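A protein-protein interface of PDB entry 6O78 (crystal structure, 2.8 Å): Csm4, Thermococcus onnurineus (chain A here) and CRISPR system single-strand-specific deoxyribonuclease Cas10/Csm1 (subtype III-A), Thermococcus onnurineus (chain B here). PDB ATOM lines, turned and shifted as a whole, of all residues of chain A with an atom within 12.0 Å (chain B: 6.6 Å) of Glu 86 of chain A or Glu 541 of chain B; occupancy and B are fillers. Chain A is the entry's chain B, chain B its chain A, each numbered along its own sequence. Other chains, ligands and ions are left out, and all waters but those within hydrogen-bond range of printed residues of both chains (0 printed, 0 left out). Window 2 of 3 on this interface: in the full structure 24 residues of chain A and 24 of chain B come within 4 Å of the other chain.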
ATOM      1  N   LEU A  77      26.879  39.205  -2.708  1.00  0.00           N
ATOM      2  CA  LEU A  77      26.323  37.873  -2.334  1.00  0.00           C
ATOM      3  C   LEU A  77      27.314  36.788  -2.772  1.00  0.00           C
ATOM      4  O   LEU A  77      27.376  35.750  -2.092  1.00  0.00           O
ATOM      5  CB  LEU A  77      24.951  37.654  -2.984  1.00  0.00           C
ATOM      6  CG  LEU A  77      23.740  38.168  -2.203  1.00  0.00           C
ATOM      7  CD1 LEU A  77      23.508  37.358  -0.941  1.00  0.00           C
ATOM      8  CD2 LEU A  77      23.889  39.635  -1.856  1.00  0.00           C
ATOM      9  N   GLU A  78      28.047  37.034  -3.856  1.00  0.00           N
ATOM     10  CA  GLU A  78      29.032  36.045  -4.359  1.00  0.00           C
ATOM     11  C   GLU A  78      30.286  36.114  -3.490  1.00  0.00           C
ATOM     12  O   GLU A  78      31.320  35.595  -3.916  1.00  0.00           O
ATOM     13  CB  GLU A  78      29.391  36.355  -5.811  1.00  0.00           C
ATOM     14  CG  GLU A  78      28.210  36.227  -6.754  1.00  0.00           C
ATOM     15  CD  GLU A  78      27.527  34.873  -6.720  1.00  0.00           C
ATOM     16  OE1 GLU A  78      27.838  34.039  -7.586  1.00  0.00           O
ATOM     17  OE2 GLU A  78      26.687  34.659  -5.829  1.00  0.00           O
ATOM     18  N   ILE A  80      29.782  36.221   0.328  1.00  0.00           N
ATOM     19  CA  ILE A  80      29.384  35.583   1.614  1.00  0.00           C
ATOM     20  C   ILE A  80      28.797  34.202   1.312  1.00  0.00           C
ATOM     21  O   ILE A  80      27.731  33.885   1.860  1.00  0.00           O
ATOM     22  CB  ILE A  80      28.388  36.475   2.375  1.00  0.00           C
ATOM     23  CG1 ILE A  80      28.865  37.927   2.416  1.00  0.00           C
ATOM     24  CG2 ILE A  80      28.134  35.924   3.768  1.00  0.00           C
ATOM     25  CD1 ILE A  80      27.779  38.933   2.153  1.00  0.00           C
ATOM     26  N   LEU A  81      29.469  33.426   0.463  1.00  0.00           N
ATOM     27  CA  LEU A  81      28.999  32.062   0.113  1.00  0.00           C
ATOM     28  C   LEU A  81      29.962  31.042   0.725  1.00  0.00           C
ATOM     29  O   LEU A  81      29.912  30.836   1.950  1.00  0.00           O
ATOM     30  CB  LEU A  81      28.960  31.921  -1.410  1.00  0.00           C
ATOM     31  CG  LEU A  81      29.639  33.038  -2.199  1.00  0.00           C
ATOM     32  CD1 LEU A  81      31.070  33.239  -1.737  1.00  0.00           C
ATOM     33  CD2 LEU A  81      29.613  32.732  -3.686  1.00  0.00           C
ATOM     34  N   THR A  82      30.811  30.442  -0.113  1.00  0.00           N
ATOM     35  CA  THR A  82      31.804  29.444   0.358  1.00  0.00           C
ATOM     36  C   THR A  82      31.082  28.370   1.178  1.00  0.00           C
ATOM     37  O   THR A  82      30.093  27.827   0.648  1.00  0.00           O
ATOM     38  CB  THR A  82      32.942  30.124   1.131  1.00  0.00           C
ATOM     39  OG1 THR A  82      33.148  31.434   0.600  1.00  0.00           O
ATOM     40  CG2 THR A  82      34.243  29.356   1.059  1.00  0.00           C
ATOM     41  N   GLU A  86      25.879  25.278  -5.026  1.00  0.00           N
ATOM     42  CA  GLU A  86      25.044  25.907  -6.086  1.00  0.00           C
ATOM     43  C   GLU A  86      23.618  26.098  -5.560  1.00  0.00           C
ATOM     44  O   GLU A  86      23.168  27.258  -5.483  1.00  0.00           O
ATOM     45  CB  GLU A  86      25.053  25.046  -7.352  1.00  0.00           C
ATOM     46  CG  GLU A  86      26.409  24.987  -8.033  1.00  0.00           C
ATOM     47  CD  GLU A  86      26.465  24.083  -9.251  1.00  0.00           C
ATOM     48  OE1 GLU A  86      25.492  23.336  -9.477  1.00  0.00           O
ATOM     49  OE2 GLU A  86      27.481  24.127  -9.973  1.00  0.00           O
ATOM     50  N   GLU A  87      22.943  24.998  -5.214  1.00  0.00           N
ATOM     51  CA  GLU A  87      21.552  25.057  -4.689  1.00  0.00           C
ATOM     52  C   GLU A  87      21.548  25.840  -3.371  1.00  0.00           C
ATOM     53  O   GLU A  87      20.645  26.679  -3.186  1.00  0.00           O
ATOM     54  CB  GLU A  87      21.012  23.642  -4.479  1.00  0.00           C
ATOM     55  CG  GLU A  87      20.947  22.824  -5.755  1.00  0.00           C
ATOM     56  CD  GLU A  87      20.364  21.431  -5.586  1.00  0.00           C
ATOM     57  OE1 GLU A  87      20.000  21.080  -4.445  1.00  0.00           O
ATOM     58  OE2 GLU A  87      20.272  20.703  -6.594  1.00  0.00           O
ATOM     59  N   GLU A  88      22.546  25.596  -2.516  1.00  0.00           N
ATOM     60  CA  GLU A  88      22.655  26.297  -1.208  1.00  0.00           C
ATOM     61  C   GLU A  88      23.174  27.720  -1.444  1.00  0.00           C
ATOM     62  O   GLU A  88      23.283  28.482  -0.463  1.00  0.00           O
ATOM     63  CB  GLU A  88      23.576  25.524  -0.262  1.00  0.00           C
ATOM     64  CG  GLU A  88      23.079  24.125   0.055  1.00  0.00           C
ATOM     65  CD  GLU A  88      21.716  24.075   0.724  1.00  0.00           C
ATOM     66  OE1 GLU A  88      21.129  25.152   0.948  1.00  0.00           O
ATOM     67  OE2 GLU A  88      21.245  22.959   1.020  1.00  0.00           O
ATOM     68  N   ARG A  89      23.482  28.051  -2.703  1.00  0.00           N
ATOM     69  CA  ARG A  89      23.995  29.400  -3.071  1.00  0.00           C
ATOM     70  C   ARG A  89      23.028  30.075  -4.055  1.00  0.00           C
ATOM     71  O   ARG A  89      23.048  31.315  -4.118  1.00  0.00           O
ATOM     72  CB  ARG A  89      25.416  29.327  -3.646  1.00  0.00           C
ATOM     73  CG  ARG A  89      25.498  28.936  -5.116  1.00  0.00           C
ATOM     74  CD  ARG A  89      26.810  29.340  -5.762  1.00  0.00           C
ATOM     75  NE  ARG A  89      26.953  28.797  -7.107  1.00  0.00           N
ATOM     76  CZ  ARG A  89      28.102  28.689  -7.774  1.00  0.00           C
ATOM     77  NH1 ARG A  89      29.241  29.082  -7.228  1.00  0.00           N
ATOM     78  NH2 ARG A  89      28.105  28.181  -8.994  1.00  0.00           N
ATOM     79  N   TYR A  90      22.237  29.298  -4.806  1.00  0.00           N
ATOM     80  CA  TYR A  90      21.194  29.808  -5.739  1.00  0.00           C
ATOM     81  C   TYR A  90      19.981  30.292  -4.938  1.00  0.00           C
ATOM     82  O   TYR A  90      19.556  31.449  -5.129  1.00  0.00           O
ATOM     83  CB  TYR A  90      20.757  28.744  -6.753  1.00  0.00           C
ATOM     84  CG  TYR A  90      21.538  28.724  -8.045  1.00  0.00           C
ATOM     85  CD1 TYR A  90      21.666  29.864  -8.824  1.00  0.00           C
ATOM     86  CD2 TYR A  90      22.123  27.557  -8.508  1.00  0.00           C
ATOM     87  CE1 TYR A  90      22.376  29.850 -10.014  1.00  0.00           C
ATOM     88  CE2 TYR A  90      22.837  27.526  -9.695  1.00  0.00           C
ATOM     89  CZ  TYR A  90      22.964  28.677 -10.453  1.00  0.00           C
ATOM     90  OH  TYR A  90      23.664  28.660 -11.624  1.00  0.00           O
ATOM     91  N   THR A  91      19.445  29.424  -4.072  1.00  0.00           N
ATOM     92  CA  THR A  91      18.163  29.625  -3.342  1.00  0.00           C
ATOM     93  C   THR A  91      18.310  30.760  -2.323  1.00  0.00           C
ATOM     94  O   THR A  91      17.528  31.724  -2.416  1.00  0.00           O
ATOM     95  CB  THR A  91      17.684  28.324  -2.687  1.00  0.00           C
ATOM     96  OG1 THR A  91      18.715  27.842  -1.824  1.00  0.00           O
ATOM     97  CG2 THR A  91      17.325  27.258  -3.700  1.00  0.00           C
ATOM     98  N   THR A  92      19.269  30.654  -1.395  1.00  0.00           N
ATOM     99  CA  THR A  92      19.503  31.649  -0.312  1.00  0.00           C
ATOM    100  C   THR A  92      19.763  33.024  -0.938  1.00  0.00           C
ATOM    101  O   THR A  92      19.018  33.961  -0.602  1.00  0.00           O
ATOM    102  CB  THR A  92      20.638  31.224   0.631  1.00  0.00           C
ATOM    103  OG1 THR A  92      21.797  30.941  -0.153  1.00  0.00           O
ATOM    104  CG2 THR A  92      20.277  30.022   1.477  1.00  0.00           C
ATOM    105  N   ALA A  93      20.749  33.123  -1.840  1.00  0.00           N
ATOM    106  CA  ALA A  93      21.143  34.366  -2.551  1.00  0.00           C
ATOM    107  C   ALA A  93      19.903  35.087  -3.098  1.00  0.00           C
ATOM    108  O   ALA A  93      19.898  36.331  -3.080  1.00  0.00           O
ATOM    109  CB  ALA A  93      22.118  34.055  -3.659  1.00  0.00           C
ATOM    110  N   LYS A  94      18.902  34.334  -3.572  1.00  0.00           N
ATOM    111  CA  LYS A  94      17.605  34.880  -4.061  1.00  0.00           C
ATOM    112  C   LYS A  94      16.767  35.373  -2.875  1.00  0.00           C
ATOM    113  O   LYS A  94      16.218  36.485  -2.974  1.00  0.00           O
ATOM    114  CB  LYS A  94      16.824  33.837  -4.870  1.00  0.00           C
ATOM    115  CG  LYS A  94      17.090  33.855  -6.368  1.00  0.00           C
ATOM    116  CD  LYS A  94      16.067  33.083  -7.172  1.00  0.00           C
ATOM    117  CE  LYS A  94      16.498  32.861  -8.606  1.00  0.00           C
ATOM    118  NZ  LYS A  94      17.470  31.747  -8.719  1.00  0.00           N
ATOM    119  N   ARG A  95      16.662  34.577  -1.804  1.00  0.00           N
ATOM    120  CA  ARG A  95      15.845  34.916  -0.605  1.00  0.00           C
ATOM    121  C   ARG A  95      16.549  36.019   0.197  1.00  0.00           C
ATOM    122  O   ARG A  95      15.850  36.727   0.947  1.00  0.00           O
ATOM    123  CB  ARG A  95      15.567  33.679   0.258  1.00  0.00           C
ATOM    124  CG  ARG A  95      14.991  32.477  -0.483  1.00  0.00           C
ATOM    125  CD  ARG A  95      13.961  32.758  -1.568  1.00  0.00           C
ATOM    126  NE  ARG A  95      12.632  33.071  -1.052  1.00  0.00           N
ATOM    127  CZ  ARG A  95      11.497  32.986  -1.748  1.00  0.00           C
ATOM    128  NH1 ARG A  95      11.504  32.585  -3.010  1.00  0.00           N
ATOM    129  NH2 ARG A  95      10.347  33.296  -1.173  1.00  0.00           N
ATOM    130  N   LEU A  96      17.872  36.165   0.045  1.00  0.00           N
ATOM    131  CA  LEU A  96      18.653  37.312   0.586  1.00  0.00           C
ATOM    132  C   LEU A  96      18.374  38.549  -0.278  1.00  0.00           C
ATOM    133  O   LEU A  96      18.169  39.632   0.300  1.00  0.00           O
ATOM    134  CB  LEU A  96      20.151  36.980   0.604  1.00  0.00           C
ATOM    135  CG  LEU A  96      20.573  35.773   1.446  1.00  0.00           C
ATOM    136  CD1 LEU A  96      22.068  35.520   1.334  1.00  0.00           C
ATOM    137  CD2 LEU A  96      20.187  35.944   2.903  1.00  0.00           C
ATOM    138  N   ARG B 538      15.010  26.609 -11.599  1.00  0.00           N
ATOM    139  CA  ARG B 538      16.493  26.544 -11.727  1.00  0.00           C
ATOM    140  C   ARG B 538      16.898  26.534 -13.207  1.00  0.00           C
ATOM    141  O   ARG B 538      17.701  25.665 -13.601  1.00  0.00           O
ATOM    142  CB  ARG B 538      17.029  25.328 -10.965  1.00  0.00           C
ATOM    143  CG  ARG B 538      17.125  25.546  -9.462  1.00  0.00           C
ATOM    144  CD  ARG B 538      17.165  24.246  -8.684  1.00  0.00           C
ATOM    145  NE  ARG B 538      17.083  24.484  -7.247  1.00  0.00           N
ATOM    146  CZ  ARG B 538      16.478  23.688  -6.365  1.00  0.00           C
ATOM    147  NH1 ARG B 538      16.474  24.018  -5.084  1.00  0.00           N
ATOM    148  NH2 ARG B 538      15.873  22.578  -6.754  1.00  0.00           N
ATOM    149  N   LEU B 539      16.361  27.477 -13.988  1.00  0.00           N
ATOM    150  CA  LEU B 539      16.756  27.729 -15.400  1.00  0.00           C
ATOM    151  C   LEU B 539      18.161  28.341 -15.429  1.00  0.00           C
ATOM    152  O   LEU B 539      18.922  28.019 -16.359  1.00  0.00           O
ATOM    153  CB  LEU B 539      15.742  28.673 -16.052  1.00  0.00           C
ATOM    154  CG  LEU B 539      15.901  28.843 -17.561  1.00  0.00           C
ATOM    155  CD1 LEU B 539      15.240  27.694 -18.301  1.00  0.00           C
ATOM    156  CD2 LEU B 539      15.338  30.174 -18.024  1.00  0.00           C
ATOM    157  N   GLY B 540      18.473  29.209 -14.462  1.00  0.00           N
ATOM    158  CA  GLY B 540      19.797  29.843 -14.306  1.00  0.00           C
ATOM    159  C   GLY B 540      20.898  28.807 -14.156  1.00  0.00           C
ATOM    160  O   GLY B 540      21.976  29.010 -14.741  1.00  0.00           O
ATOM    161  N   GLU B 541      20.624  27.735 -13.406  1.00  0.00           N
ATOM    162  CA  GLU B 541      21.543  26.586 -13.181  1.00  0.00           C
ATOM    163  C   GLU B 541      21.684  25.786 -14.482  1.00  0.00           C
ATOM    164  O   GLU B 541      22.823  25.405 -14.821  1.00  0.00           O
ATOM    165  CB  GLU B 541      21.011  25.714 -12.040  1.00  0.00           C
ATOM    166  CG  GLU B 541      22.000  24.673 -11.547  1.00  0.00           C
ATOM    167  CD  GLU B 541      21.708  24.110 -10.164  1.00  0.00           C
ATOM    168  OE1 GLU B 541      20.851  24.682  -9.455  1.00  0.00           O
ATOM    169  OE2 GLU B 541      22.339  23.099  -9.796  1.00  0.00           O
ATOM    170  N   PHE B 542      20.565  25.552 -15.178  1.00  0.00           N
ATOM    171  CA  PHE B 542      20.476  24.790 -16.453  1.00  0.00           C
ATOM    172  C   PHE B 542      21.367  25.449 -17.514  1.00  0.00           C
ATOM    173  O   PHE B 542      22.275  24.774 -18.035  1.00  0.00           O
ATOM    174  CB  PHE B 542      19.019  24.699 -16.913  1.00  0.00           C
ATOM    175  CG  PHE B 542      18.805  24.004 -18.234  1.00  0.00           C
ATOM    176  CD1 PHE B 542      19.139  22.667 -18.397  1.00  0.00           C
ATOM    177  CD2 PHE B 542      18.253  24.682 -19.312  1.00  0.00           C
ATOM    178  CE1 PHE B 542      18.935  22.028 -19.610  1.00  0.00           C
ATOM    179  CE2 PHE B 542      18.048  24.040 -20.525  1.00  0.00           C
ATOM    180  CZ  PHE B 542      18.389  22.715 -20.671  1.00  0.00           C
ATOM    181  N   PHE B 543      21.117  26.729 -17.813  1.00  0.00           N
ATOM    182  CA  PHE B 543      21.871  27.535 -18.812  1.00  0.00           C
ATOM    183  C   PHE B 543      23.355  27.608 -18.427  1.00  0.00           C
ATOM    184  O   PHE B 543      24.206  27.633 -19.338  1.00  0.00           O
ATOM    185  CB  PHE B 543      21.292  28.949 -18.939  1.00  0.00           C
ATOM    186  CG  PHE B 543      19.958  29.061 -19.638  1.00  0.00           C
ATOM    187  CD1 PHE B 543      19.540  28.122 -20.571  1.00  0.00           C
ATOM    188  CD2 PHE B 543      19.133  30.146 -19.389  1.00  0.00           C
ATOM    189  CE1 PHE B 543      18.317  28.252 -21.213  1.00  0.00           C
ATOM    190  CE2 PHE B 543      17.913  30.277 -20.034  1.00  0.00           C
ATOM    191  CZ  PHE B 543      17.505  29.329 -20.943  1.00  0.00           C
ATOM    192  N   SER B 544      23.655  27.646 -17.124  1.00  0.00           N
ATOM    193  CA  SER B 544      25.030  27.766 -16.572  1.00  0.00           C
ATOM    194  C   SER B 544      25.822  26.469 -16.800  1.00  0.00           C
ATOM    195  O   SER B 544      27.065  26.521 -16.704  1.00  0.00           O
ATOM    196  CB  SER B 544      24.997  28.140 -15.112  1.00  0.00           C
ATOM    197  OG  SER B 544      26.294  28.481 -14.648  1.00  0.00           O
ATOM    198  N   SER B 545      25.137  25.354 -17.083  1.00  0.00           N
ATOM    199  CA  SER B 545      25.748  24.023 -17.346  1.00  0.00           C
ATOM    200  C   SER B 545      26.204  23.913 -18.808  1.00  0.00           C
ATOM    201  O   SER B 545      27.027  23.019 -19.092  1.00  0.00           O
ATOM    202  CB  SER B 545      24.800  22.905 -16.983  1.00  0.00           C
ATOM    203  OG  SER B 545      23.773  22.767 -17.955  1.00  0.00           O
ATOM    204  N   MET B 546      25.692  24.774 -19.699  1.00  0.00           N
ATOM    205  CA  MET B 546      26.021  24.763 -21.152  1.00  0.00           C
ATOM    206  C   MET B 546      27.474  25.220 -21.344  1.00  0.00           C
ATOM    207  O   MET B 546      27.827  26.304 -20.840  1.00  0.00           O
ATOM    208  CB  MET B 546      25.091  25.678 -21.958  1.00  0.00           C
ATOM    209  CG  MET B 546      23.601  25.413 -21.757  1.00  0.00           C
ATOM    210  SD  MET B 546      23.166  23.690 -21.372  1.00  0.00           S
ATOM    211  CE  MET B 546      23.100  22.977 -23.013  1.00  0.00           C
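The side-chain carboxylate (OE2) of Glu 541 of chain B sits close to the side-chain carboxylate (OE1) of Glu 86 of chain A.
The backbone carbonyl oxygen (O) of Glu 87 of chain A lies within hydrogen-bond range of the side-chain hydroxyl (OG1) of Thr 91 of chain A, at 2.6 Å.
Tyr 90 of chain A touches Gly 540 of chain B (OH to O, 3.6 Å).
Glu 541 of chain B touches Tyr 90 of chain A.
CB of Ser 544 of chain B touches OH of Tyr 90 of chain A (3.8 Å).
NH1 of Arg 538 of chain B touches CG2 of Thr 91 of chain A, 3.6 Å away.
Arg 538 of chain B touches just one residue of chain A: Thr 91 (3.6 Å).
No residue of chain A comes within 4 Å of Leu 539 of chain B.
Printed residues of chain A within 4 Å of Gly 540 of chain B: Tyr 90 (3.6 Å).
Ser 544 of chain B touches just one residue of chain A: Tyr 90.
No residue of chain A comes within 4 Å of Ser 545 of chain B.
Of the printed residues of chain B, Thr 91 of chain A touches Arg 538 (3.6 Å).
Of the printed residues of chain B, Tyr 90 of chain A touches Gly 540, Glu 541 and Ser 544.
The nearest residue of chain B that does not touch Glu 86 of chain A is Ser 544 of chain B (6.5 Å).
The nearest residue of chain A that does not touch Glu 541 of chain B is Glu 87 of chain A (4.1 Å).
The nearest printed residue of chain B that does not touch Tyr 90 of chain A is Arg 538 of chain B (5.5 Å).
Hydrophobic or aromatic side chains of chain A that line the printed part of chain B: Tyr 90.
Of the 9 printed residues of chain B, 4 touch a printed residue of chain A.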
